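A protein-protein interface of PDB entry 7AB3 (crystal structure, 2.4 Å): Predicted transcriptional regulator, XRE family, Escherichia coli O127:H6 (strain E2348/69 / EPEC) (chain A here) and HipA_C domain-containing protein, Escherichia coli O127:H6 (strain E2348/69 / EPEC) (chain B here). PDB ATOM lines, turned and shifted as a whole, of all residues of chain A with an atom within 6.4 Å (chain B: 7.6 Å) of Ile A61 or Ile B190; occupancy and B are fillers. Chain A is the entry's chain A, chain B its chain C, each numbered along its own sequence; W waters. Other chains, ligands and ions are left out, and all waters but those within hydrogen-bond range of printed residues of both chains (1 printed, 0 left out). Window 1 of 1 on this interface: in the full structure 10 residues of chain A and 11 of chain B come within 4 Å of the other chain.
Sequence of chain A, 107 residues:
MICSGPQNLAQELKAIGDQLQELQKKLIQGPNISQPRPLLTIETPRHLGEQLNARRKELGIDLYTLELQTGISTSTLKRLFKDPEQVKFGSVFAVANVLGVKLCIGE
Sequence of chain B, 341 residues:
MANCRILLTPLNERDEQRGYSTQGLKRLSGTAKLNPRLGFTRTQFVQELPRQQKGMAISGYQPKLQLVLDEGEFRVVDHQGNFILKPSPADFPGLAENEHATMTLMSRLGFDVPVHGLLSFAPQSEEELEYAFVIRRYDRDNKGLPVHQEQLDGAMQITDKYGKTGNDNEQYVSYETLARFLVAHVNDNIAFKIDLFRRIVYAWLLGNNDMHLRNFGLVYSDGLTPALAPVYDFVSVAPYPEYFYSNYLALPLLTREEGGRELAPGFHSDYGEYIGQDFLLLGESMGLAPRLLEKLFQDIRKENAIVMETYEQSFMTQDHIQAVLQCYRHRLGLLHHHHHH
The backbone carbonyl oxygen (O) of Gly A100 lies within hydrogen-bond range of the side-chain amide nitrogen (ND2) of Asn B187, at 2.9 Å. The guanidinium group of Arg A55 sits at hydrogen-bond distance from the side-chain amide oxygen of Asn B187 (2.7 Å). The side-chain amide nitrogen (NE2) of Gln A69 is in hydrogen-bond range of the backbone carbonyl oxygen (O) of Gly B287 (2.9 Å). The backbone carbonyl oxygen (O) of Val A98 sits at hydrogen-bond distance from the backbone NH (N) of Ile B190, at 3.0 Å. The side-chain amide oxygen of Gln A69 sits at hydrogen-bond distance from the backbone NH of Ala B289, 2.8 Å away.
OD1 of Asn B187 sits at hydrogen-bond distance from ND2 of Asn B189 (2.8 Å). The side-chain amide oxygen (OD1) of Asn B189 sits at hydrogen-bond distance from the backbone NH (N) of Ala B191. The side-chain amide oxygen of Asn B189 lies within hydrogen-bond range of the backbone NH of Phe B192, at 3.1 Å. NH1 of Arg A55 is in salt-bridge range of OE1 of Glu A58, at 2.9 Å. NH1 of Arg A56 lies within hydrogen-bond range of O of Ile A61. The side-chain carboxylate (OD1) of Asp A62 is in hydrogen-bond range of the side-chain hydroxyl (OG1) of Thr A65.
NH2 of Arg A55 touches ND2 of Asn B189, at 3.8 Å. CD1 of Leu A59 touches CG of Asn B189 (3.8 Å). Ala B191 touches Leu A59 (CB to O, 3.6 Å). Ala B191 touches Ile A61 (CB to CG1, 3.9 Å). Thr A65 touches Leu B292 (CG2 to CD1, 3.98 Å). Leu B288 touches Gln A69. Leu B292 touches Gln A69 (CD2 to OE1, 3.3 Å). O of Val A98 touches CA of Asn B189 (3.1 Å). Leu A99 touches Asn B189. CB of Asn B189 touches N of Gly A100 (3.9 Å).
Of chain B, only Ile B190 and Ala B191 come within 4 Å of Ile A61. Ile B190 touches just these residues of chain A: Ile A61, Gln A69 and Val A98. Of the printed residues of chain B, Leu A59 touches Asn B189 (3.8 Å) and Ala B191 (3.6 Å). Printed residues of chain A within 4 Å of Asn B189: Arg A55 (3.8 Å), Leu A59 (3.8 Å), Val A98 (3.1 Å), Leu A99 (3.6 Å) and Gly A100 (3.9 Å). Printed residues of chain B within 4 Å of Val A98: Asn B189 (3.1 Å) and Ile B190 (3.0 Å). Of the printed residues of chain A, Ile B194 touches Thr A65. Lys B193 touches none of the printed residues of chain A. Leu A63 touches none of the printed residues of chain B. The nearest residue of chain B that does not touch Ile A61 is Asn B189 (5.0 Å). The nearest residue of chain A that does not touch Ile B190 is Thr A65 (4.6 Å).
Of the 16 printed residues of chain A, 8 touch a printed residue of chain B. Hydrophobic or aromatic side chains of chain A within 4 Å of the printed part of chain B: Leu A59, Ile A61 and Val A98. Along chain A the printed residues that touch a printed residue of chain B span positions 55 to 100. Hydrophobic or aromatic side chains of chain B that line the printed part of chain A: Ile B190, Ala B191, Ile B194, Ala B289 and Leu B292. Along chain B the printed residues that touch a printed residue of chain A span positions 187 to 292. Among the printed residues, no Asp or Glu carboxylate lies within 4 Å of a Lys or Arg side-chain nitrogen of the other chain.
Water W1 bridges the side-chain amino group (NZ) of Lys B193 and the backbone carbonyl oxygen (O) of Asn A97.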
ATOM      1  N   ARG A  55     -31.493 -18.955  -3.492  1.00  0.00           N
ATOM      2  CA  ARG A  55     -30.674 -19.460  -2.401  1.00  0.00           C
ATOM      3  C   ARG A  55     -29.653 -18.413  -1.983  1.00  0.00           C
ATOM      4  O   ARG A  55     -29.452 -18.201  -0.789  1.00  0.00           O
ATOM      5  CB  ARG A  55     -29.965 -20.756  -2.855  1.00  0.00           C
ATOM      6  CG  ARG A  55     -28.981 -21.321  -1.869  1.00  0.00           C
ATOM      7  CD  ARG A  55     -29.631 -21.773  -0.587  1.00  0.00           C
ATOM      8  NE  ARG A  55     -28.662 -22.454   0.270  1.00  0.00           N
ATOM      9  CZ  ARG A  55     -28.854 -22.727   1.556  1.00  0.00           C
ATOM     10  NH1 ARG A  55     -29.982 -22.369   2.160  1.00  0.00           N
ATOM     11  NH2 ARG A  55     -27.914 -23.335   2.254  1.00  0.00           N
ATOM     12  N   ARG A  56     -28.995 -17.764  -2.963  1.00  0.00           N
ATOM     13  CA  ARG A  56     -28.016 -16.706  -2.731  1.00  0.00           C
ATOM     14  C   ARG A  56     -28.628 -15.542  -1.956  1.00  0.00           C
ATOM     15  O   ARG A  56     -28.037 -15.066  -0.991  1.00  0.00           O
ATOM     16  CB  ARG A  56     -27.451 -16.216  -4.069  1.00  0.00           C
ATOM     17  CG  ARG A  56     -26.372 -15.170  -3.890  1.00  0.00           C
ATOM     18  CD  ARG A  56     -26.005 -14.477  -5.179  1.00  0.00           C
ATOM     19  NE  ARG A  56     -27.149 -13.845  -5.833  1.00  0.00           N
ATOM     20  CZ  ARG A  56     -27.551 -12.600  -5.599  1.00  0.00           C
ATOM     21  NH1 ARG A  56     -26.918 -11.844  -4.708  1.00  0.00           N
ATOM     22  NH2 ARG A  56     -28.606 -12.112  -6.229  1.00  0.00           N
ATOM     23  N   LYS A  57     -29.819 -15.108  -2.356  1.00  0.00           N
ATOM     24  CA  LYS A  57     -30.525 -14.017  -1.711  1.00  0.00           C
ATOM     25  C   LYS A  57     -31.029 -14.371  -0.311  1.00  0.00           C
ATOM     26  O   LYS A  57     -31.040 -13.490   0.545  1.00  0.00           O
ATOM     27  CB  LYS A  57     -31.694 -13.533  -2.580  1.00  0.00           C
ATOM     28  CG  LYS A  57     -31.273 -12.922  -3.899  1.00  0.00           C
ATOM     29  CD  LYS A  57     -32.489 -12.648  -4.764  1.00  0.00           C
ATOM     30  CE  LYS A  57     -32.043 -11.987  -6.047  1.00  0.00           C
ATOM     31  NZ  LYS A  57     -33.166 -11.600  -6.929  1.00  0.00           N
ATOM     32  N   GLU A  58     -31.459 -15.626  -0.059  1.00  0.00           N
ATOM     33  CA  GLU A  58     -31.916 -16.013   1.289  1.00  0.00           C
ATOM     34  C   GLU A  58     -30.745 -16.111   2.302  1.00  0.00           C
ATOM     35  O   GLU A  58     -30.952 -15.986   3.514  1.00  0.00           O
ATOM     36  CB  GLU A  58     -32.784 -17.280   1.268  1.00  0.00           C
ATOM     37  CG  GLU A  58     -32.027 -18.592   1.336  1.00  0.00           C
ATOM     38  CD  GLU A  58     -32.878 -19.827   1.109  1.00  0.00           C
ATOM     39  OE1 GLU A  58     -32.444 -20.931   1.513  1.00  0.00           O
ATOM     40  OE2 GLU A  58     -33.971 -19.695   0.508  1.00  0.00           O
ATOM     41  N   LEU A  59     -29.519 -16.311   1.799  1.00  0.00           N
ATOM     42  CA  LEU A  59     -28.304 -16.335   2.607  1.00  0.00           C
ATOM     43  C   LEU A  59     -27.693 -14.946   2.788  1.00  0.00           C
ATOM     44  O   LEU A  59     -26.790 -14.790   3.601  1.00  0.00           O
ATOM     45  CB  LEU A  59     -27.263 -17.287   1.998  1.00  0.00           C
ATOM     46  CG  LEU A  59     -27.607 -18.769   2.005  1.00  0.00           C
ATOM     47  CD1 LEU A  59     -26.562 -19.557   1.274  1.00  0.00           C
ATOM     48  CD2 LEU A  59     -27.809 -19.276   3.405  1.00  0.00           C
ATOM     49  N   GLY A  60     -28.197 -13.939   2.067  1.00  0.00           N
ATOM     50  CA  GLY A  60     -27.723 -12.568   2.138  1.00  0.00           C
ATOM     51  C   GLY A  60     -26.379 -12.363   1.473  1.00  0.00           C
ATOM     52  O   GLY A  60     -25.652 -11.432   1.823  1.00  0.00           O
ATOM     53  N   ILE A  61     -26.032 -13.211   0.507  1.00  0.00           N
ATOM     54  CA  ILE A  61     -24.754 -13.152  -0.188  1.00  0.00           C
ATOM     55  C   ILE A  61     -24.865 -12.287  -1.417  1.00  0.00           C
ATOM     56  O   ILE A  61     -25.776 -12.464  -2.215  1.00  0.00           O
ATOM     57  CB  ILE A  61     -24.223 -14.574  -0.535  1.00  0.00           C
ATOM     58  CG1 ILE A  61     -24.130 -15.468   0.706  1.00  0.00           C
ATOM     59  CG2 ILE A  61     -22.900 -14.538  -1.288  1.00  0.00           C
ATOM     60  CD1 ILE A  61     -24.109 -16.918   0.347  1.00  0.00           C
ATOM     61  N   ASP A  62     -23.968 -11.317  -1.552  1.00  0.00           N
ATOM     62  CA  ASP A  62     -23.951 -10.466  -2.725  1.00  0.00           C
ATOM     63  C   ASP A  62     -23.028 -11.057  -3.809  1.00  0.00           C
ATOM     64  O   ASP A  62     -22.284 -11.997  -3.546  1.00  0.00           O
ATOM     65  CB  ASP A  62     -23.627  -9.006  -2.354  1.00  0.00           C
ATOM     66  CG  ASP A  62     -22.242  -8.755  -1.807  1.00  0.00           C
ATOM     67  OD1 ASP A  62     -21.452  -9.708  -1.732  1.00  0.00           O
ATOM     68  OD2 ASP A  62     -21.945  -7.594  -1.467  1.00  0.00           O
ATOM     69  N   LEU A  63     -23.107 -10.528  -5.031  1.00  0.00           N
ATOM     70  CA  LEU A  63     -22.314 -10.977  -6.171  1.00  0.00           C
ATOM     71  C   LEU A  63     -20.827 -10.732  -5.993  1.00  0.00           C
ATOM     72  O   LEU A  63     -20.030 -11.515  -6.479  1.00  0.00           O
ATOM     73  CB  LEU A  63     -22.820 -10.288  -7.447  1.00  0.00           C
ATOM     74  CG  LEU A  63     -24.226 -10.667  -7.849  1.00  0.00           C
ATOM     75  CD1 LEU A  63     -24.728  -9.772  -8.977  1.00  0.00           C
ATOM     76  CD2 LEU A  63     -24.295 -12.096  -8.245  1.00  0.00           C
ATOM     77  N   THR A  65     -19.107 -10.858  -3.107  1.00  0.00           N
ATOM     78  CA  THR A  65     -18.579 -11.879  -2.191  1.00  0.00           C
ATOM     79  C   THR A  65     -18.281 -13.175  -2.920  1.00  0.00           C
ATOM     80  O   THR A  65     -17.247 -13.789  -2.669  1.00  0.00           O
ATOM     81  CB  THR A  65     -19.521 -12.114  -0.991  1.00  0.00           C
ATOM     82  OG1 THR A  65     -19.665 -10.897  -0.249  1.00  0.00           O
ATOM     83  CG2 THR A  65     -19.032 -13.223  -0.074  1.00  0.00           C
ATOM     84  N   LEU A  66     -19.176 -13.561  -3.847  1.00  0.00           N
ATOM     85  CA  LEU A  66     -19.063 -14.742  -4.694  1.00  0.00           C
ATOM     86  C   LEU A  66     -17.905 -14.630  -5.688  1.00  0.00           C
ATOM     87  O   LEU A  66     -17.300 -15.632  -6.045  1.00  0.00           O
ATOM     88  CB  LEU A  66     -20.364 -14.913  -5.490  1.00  0.00           C
ATOM     89  CG  LEU A  66     -21.588 -15.426  -4.758  1.00  0.00           C
ATOM     90  CD1 LEU A  66     -22.714 -15.600  -5.708  1.00  0.00           C
ATOM     91  CD2 LEU A  66     -21.323 -16.744  -4.132  1.00  0.00           C
ATOM     92  N   GLN A  69     -14.595 -15.196  -3.748  1.00  0.00           N
ATOM     93  CA  GLN A  69     -14.476 -16.582  -3.313  1.00  0.00           C
ATOM     94  C   GLN A  69     -14.279 -17.586  -4.458  1.00  0.00           C
ATOM     95  O   GLN A  69     -13.545 -18.553  -4.316  1.00  0.00           O
ATOM     96  CB  GLN A  69     -15.721 -16.952  -2.477  1.00  0.00           C
ATOM     97  CG  GLN A  69     -15.757 -18.403  -1.993  1.00  0.00           C
ATOM     98  CD  GLN A  69     -14.613 -18.777  -1.104  1.00  0.00           C
ATOM     99  OE1 GLN A  69     -14.023 -17.945  -0.419  1.00  0.00           O
ATOM    100  NE2 GLN A  69     -14.281 -20.045  -1.064  1.00  0.00           N
ATOM    101  N   ASN A  97     -21.835 -25.038  -4.820  1.00  0.00           N
ATOM    102  CA  ASN A  97     -21.027 -25.431  -3.687  1.00  0.00           C
ATOM    103  C   ASN A  97     -20.919 -24.352  -2.597  1.00  0.00           C
ATOM    104  O   ASN A  97     -21.223 -24.626  -1.434  1.00  0.00           O
ATOM    105  CB  ASN A  97     -19.672 -25.807  -4.195  1.00  0.00           C
ATOM    106  CG  ASN A  97     -19.267 -27.132  -3.669  1.00  0.00           C
ATOM    107  OD1 ASN A  97     -18.763 -27.227  -2.533  1.00  0.00           O
ATOM    108  ND2 ASN A  97     -19.531 -28.184  -4.471  1.00  0.00           N
ATOM    109  N   VAL A  98     -20.529 -23.127  -2.972  1.00  0.00           N
ATOM    110  CA  VAL A  98     -20.439 -21.981  -2.079  1.00  0.00           C
ATOM    111  C   VAL A  98     -21.799 -21.635  -1.435  1.00  0.00           C
ATOM    112  O   VAL A  98     -21.811 -21.058  -0.352  1.00  0.00           O
ATOM    113  CB  VAL A  98     -19.786 -20.803  -2.855  1.00  0.00           C
ATOM    114  CG1 VAL A  98     -20.357 -19.444  -2.513  1.00  0.00           C
ATOM    115  CG2 VAL A  98     -18.282 -20.834  -2.741  1.00  0.00           C
ATOM    116  N   LEU A  99     -22.926 -21.977  -2.092  1.00  0.00           N
ATOM    117  CA  LEU A  99     -24.273 -21.743  -1.567  1.00  0.00           C
ATOM    118  C   LEU A  99     -24.802 -22.877  -0.689  1.00  0.00           C
ATOM    119  O   LEU A  99     -25.889 -22.733  -0.145  1.00  0.00           O
ATOM    120  CB  LEU A  99     -25.283 -21.466  -2.699  1.00  0.00           C
ATOM    121  CG  LEU A  99     -24.998 -20.251  -3.598  1.00  0.00           C
ATOM    122  CD1 LEU A  99     -25.875 -20.247  -4.804  1.00  0.00           C
ATOM    123  CD2 LEU A  99     -25.032 -18.958  -2.832  1.00  0.00           C
ATOM    124  N   GLY A 100     -24.064 -23.987  -0.561  1.00  0.00           N
ATOM    125  CA  GLY A 100     -24.484 -25.135   0.239  1.00  0.00           C
ATOM    126  C   GLY A 100     -25.525 -26.006  -0.446  1.00  0.00           C
ATOM    127  O   GLY A 100     -26.290 -26.721   0.211  1.00  0.00           O
ATOM    128  N   ASN B 187     -25.359 -26.716   7.383  1.00  0.00           N
ATOM    129  CA  ASN B 187     -25.167 -26.452   5.957  1.00  0.00           C
ATOM    130  C   ASN B 187     -23.896 -25.575   5.784  1.00  0.00           C
ATOM    131  O   ASN B 187     -23.707 -24.563   6.467  1.00  0.00           O
ATOM    132  CB  ASN B 187     -26.369 -25.766   5.335  1.00  0.00           C
ATOM    133  CG  ASN B 187     -26.215 -25.561   3.865  1.00  0.00           C
ATOM    134  OD1 ASN B 187     -25.755 -24.524   3.406  1.00  0.00           O
ATOM    135  ND2 ASN B 187     -26.596 -26.544   3.090  1.00  0.00           N
ATOM    136  N   ASP B 188     -23.054 -26.005   4.853  1.00  0.00           N
ATOM    137  CA  ASP B 188     -21.777 -25.420   4.525  1.00  0.00           C
ATOM    138  C   ASP B 188     -21.864 -23.937   4.222  1.00  0.00           C
ATOM    139  O   ASP B 188     -21.646 -23.150   5.136  1.00  0.00           O
ATOM    140  CB  ASP B 188     -21.106 -26.224   3.388  1.00  0.00           C
ATOM    141  CG  ASP B 188     -19.713 -26.700   3.718  1.00  0.00           C
ATOM    142  OD1 ASP B 188     -19.341 -26.654   4.906  1.00  0.00           O
ATOM    143  OD2 ASP B 188     -18.991 -27.130   2.783  1.00  0.00           O
ATOM    144  N   ASN B 189     -22.161 -23.538   2.980  1.00  0.00           N
ATOM    145  CA  ASN B 189     -22.269 -22.157   2.523  1.00  0.00           C
ATOM    146  C   ASN B 189     -21.283 -21.114   3.188  1.00  0.00           C
ATOM    147  O   ASN B 189     -20.966 -21.122   4.396  1.00  0.00           O
ATOM    148  CB  ASN B 189     -23.722 -21.667   2.547  1.00  0.00           C
ATOM    149  CG  ASN B 189     -24.325 -21.165   3.828  1.00  0.00           C
ATOM    150  OD1 ASN B 189     -24.125 -20.025   4.222  1.00  0.00           O
ATOM    151  ND2 ASN B 189     -25.154 -21.952   4.459  1.00  0.00           N
ATOM    152  N   ILE B 190     -20.826 -20.201   2.319  1.00  0.00           N
ATOM    153  CA  ILE B 190     -19.904 -19.114   2.586  1.00  0.00           C
ATOM    154  C   ILE B 190     -20.439 -18.064   3.575  1.00  0.00           C
ATOM    155  O   ILE B 190     -19.635 -17.445   4.261  1.00  0.00           O
ATOM    156  CB  ILE B 190     -19.470 -18.485   1.250  1.00  0.00           C
ATOM    157  CG1 ILE B 190     -18.109 -17.844   1.373  1.00  0.00           C
ATOM    158  CG2 ILE B 190     -20.514 -17.533   0.666  1.00  0.00           C
ATOM    159  CD1 ILE B 190     -17.083 -18.861   1.471  1.00  0.00           C
ATOM    160  N   ALA B 191     -21.768 -17.908   3.705  1.00  0.00           N
ATOM    161  CA  ALA B 191     -22.339 -16.973   4.661  1.00  0.00           C
ATOM    162  C   ALA B 191     -22.121 -17.451   6.098  1.00  0.00           C
ATOM    163  O   ALA B 191     -21.718 -16.665   6.954  1.00  0.00           O
ATOM    164  CB  ALA B 191     -23.822 -16.753   4.363  1.00  0.00           C
ATOM    165  N   PHE B 192     -22.323 -18.753   6.341  1.00  0.00           N
ATOM    166  CA  PHE B 192     -22.103 -19.421   7.633  1.00  0.00           C
ATOM    167  C   PHE B 192     -20.606 -19.336   8.008  1.00  0.00           C
ATOM    168  O   PHE B 192     -20.254 -19.083   9.161  1.00  0.00           O
ATOM    169  CB  PHE B 192     -22.592 -20.909   7.558  1.00  0.00           C
ATOM    170  CG  PHE B 192     -21.867 -21.836   8.512  1.00  0.00           C
ATOM    171  CD1 PHE B 192     -22.121 -21.795   9.873  1.00  0.00           C
ATOM    172  CD2 PHE B 192     -20.843 -22.655   8.068  1.00  0.00           C
ATOM    173  CE1 PHE B 192     -21.357 -22.535  10.763  1.00  0.00           C
ATOM    174  CE2 PHE B 192     -20.093 -23.408   8.962  1.00  0.00           C
ATOM    175  CZ  PHE B 192     -20.355 -23.336  10.302  1.00  0.00           C
ATOM    176  N   LYS B 193     -19.737 -19.597   7.030  1.00  0.00           N
ATOM    177  CA  LYS B 193     -18.293 -19.627   7.185  1.00  0.00           C
ATOM    178  C   LYS B 193     -17.716 -18.267   7.469  1.00  0.00           C
ATOM    179  O   LYS B 193     -16.782 -18.177   8.256  1.00  0.00           O
ATOM    180  CB  LYS B 193     -17.635 -20.198   5.929  1.00  0.00           C
ATOM    181  CG  LYS B 193     -17.740 -21.691   5.772  1.00  0.00           C
ATOM    182  CD  LYS B 193     -17.270 -22.030   4.386  1.00  0.00           C
ATOM    183  CE  LYS B 193     -17.208 -23.499   4.133  1.00  0.00           C
ATOM    184  NZ  LYS B 193     -16.405 -23.754   2.916  1.00  0.00           N
ATOM    185  N   ILE B 194     -18.186 -17.218   6.765  1.00  0.00           N
ATOM    186  CA  ILE B 194     -17.723 -15.852   6.987  1.00  0.00           C
ATOM    187  C   ILE B 194     -18.151 -15.415   8.394  1.00  0.00           C
ATOM    188  O   ILE B 194     -17.353 -14.849   9.118  1.00  0.00           O
ATOM    189  CB  ILE B 194     -18.272 -14.902   5.898  1.00  0.00           C
ATOM    190  CG1 ILE B 194     -17.592 -15.158   4.546  1.00  0.00           C
ATOM    191  CG2 ILE B 194     -18.118 -13.417   6.314  1.00  0.00           C
ATOM    192  CD1 ILE B 194     -18.306 -14.447   3.388  1.00  0.00           C
ATOM    193  N   ASP B 195     -19.378 -15.731   8.803  1.00  0.00           N
ATOM    194  CA  ASP B 195     -19.880 -15.352  10.127  1.00  0.00           C
ATOM    195  C   ASP B 195     -19.096 -15.998  11.257  1.00  0.00           C
ATOM    196  O   ASP B 195     -18.645 -15.291  12.155  1.00  0.00           O
ATOM    197  CB  ASP B 195     -21.387 -15.655  10.231  1.00  0.00           C
ATOM    198  CG  ASP B 195     -22.012 -15.300  11.575  1.00  0.00           C
ATOM    199  OD1 ASP B 195     -22.539 -14.146  11.713  1.00  0.00           O
ATOM    200  OD2 ASP B 195     -22.044 -16.187  12.468  1.00  0.00           O
ATOM    201  N   LEU B 196     -18.905 -17.327  11.208  1.00  0.00           N
ATOM    202  CA  LEU B 196     -18.181 -18.077  12.211  1.00  0.00           C
ATOM    203  C   LEU B 196     -16.728 -17.607  12.291  1.00  0.00           C
ATOM    204  O   LEU B 196     -16.186 -17.474  13.391  1.00  0.00           O
ATOM    205  CB  LEU B 196     -18.259 -19.574  11.868  1.00  0.00           C
ATOM    206  CG  LEU B 196     -17.398 -20.512  12.713  1.00  0.00           C
ATOM    207  CD1 LEU B 196     -17.809 -20.470  14.164  1.00  0.00           C
ATOM    208  CD2 LEU B 196     -17.474 -21.888  12.189  1.00  0.00           C
ATOM    209  N   MET B 286     -11.067 -23.239   6.677  1.00  0.00           N
ATOM    210  CA  MET B 286     -12.522 -23.211   6.500  1.00  0.00           C
ATOM    211  C   MET B 286     -12.937 -23.124   5.014  1.00  0.00           C
ATOM    212  O   MET B 286     -14.127 -23.041   4.734  1.00  0.00           O
ATOM    213  CB  MET B 286     -13.145 -22.036   7.284  1.00  0.00           C
ATOM    214  CG  MET B 286     -12.855 -22.076   8.772  1.00  0.00           C
ATOM    215  SD  MET B 286     -13.450 -20.608   9.655  1.00  0.00           S
ATOM    216  CE  MET B 286     -15.175 -20.871   9.531  1.00  0.00           C
ATOM    217  N   GLY B 287     -11.978 -23.118   4.089  1.00  0.00           N
ATOM    218  CA  GLY B 287     -12.264 -23.019   2.669  1.00  0.00           C
ATOM    219  C   GLY B 287     -12.395 -21.605   2.138  1.00  0.00           C
ATOM    220  O   GLY B 287     -12.706 -21.437   0.960  1.00  0.00           O
ATOM    221  N   LEU B 288     -12.159 -20.568   2.972  1.00  0.00           N
ATOM    222  CA  LEU B 288     -12.275 -19.181   2.506  1.00  0.00           C
ATOM    223  C   LEU B 288     -11.083 -18.816   1.613  1.00  0.00           C
ATOM    224  O   LEU B 288      -9.953 -19.184   1.912  1.00  0.00           O
ATOM    225  CB  LEU B 288     -12.473 -18.167   3.650  1.00  0.00           C
ATOM    226  CG  LEU B 288     -13.525 -18.500   4.704  1.00  0.00           C
ATOM    227  CD1 LEU B 288     -13.318 -17.667   5.945  1.00  0.00           C
ATOM    228  CD2 LEU B 288     -14.909 -18.307   4.181  1.00  0.00           C
ATOM    229  N   ALA B 289     -11.349 -18.128   0.495  1.00  0.00           N
ATOM    230  CA  ALA B 289     -10.341 -17.790  -0.497  1.00  0.00           C
ATOM    231  C   ALA B 289      -9.503 -16.624  -0.066  1.00  0.00           C
ATOM    232  O   ALA B 289     -10.024 -15.707   0.574  1.00  0.00           O
ATOM    233  CB  ALA B 289     -11.000 -17.496  -1.831  1.00  0.00           C
ATOM    234  N   LEU B 292     -10.999 -13.250  -0.688  1.00  0.00           N
ATOM    235  CA  LEU B 292     -12.124 -13.022   0.198  1.00  0.00           C
ATOM    236  C   LEU B 292     -11.629 -12.675   1.633  1.00  0.00           C
ATOM    237  O   LEU B 292     -12.129 -11.732   2.224  1.00  0.00           O
ATOM    238  CB  LEU B 292     -13.100 -14.224   0.201  1.00  0.00           C
ATOM    239  CG  LEU B 292     -14.268 -14.055   1.176  1.00  0.00           C
ATOM    240  CD1 LEU B 292     -15.164 -12.879   0.798  1.00  0.00           C
ATOM    241  CD2 LEU B 292     -14.999 -15.305   1.388  1.00  0.00           C
ATOM    242  N   LEU B 296     -12.341  -9.395   3.899  1.00  0.00           N
ATOM    243  CA  LEU B 296     -12.897  -9.544   5.243  1.00  0.00           C
ATOM    244  C   LEU B 296     -12.070  -8.774   6.268  1.00  0.00           C
ATOM    245  O   LEU B 296     -12.644  -8.229   7.210  1.00  0.00           O
ATOM    246  CB  LEU B 296     -12.962 -11.046   5.631  1.00  0.00           C
ATOM    247  CG  LEU B 296     -13.950 -11.918   4.854  1.00  0.00           C
ATOM    248  CD1 LEU B 296     -13.946 -13.376   5.359  1.00  0.00           C
ATOM    249  CD2 LEU B 296     -15.371 -11.282   4.786  1.00  0.00           C
HETATM  250  O   HOH W   1     -19.056 -23.841   1.046  1.00  0.00           O
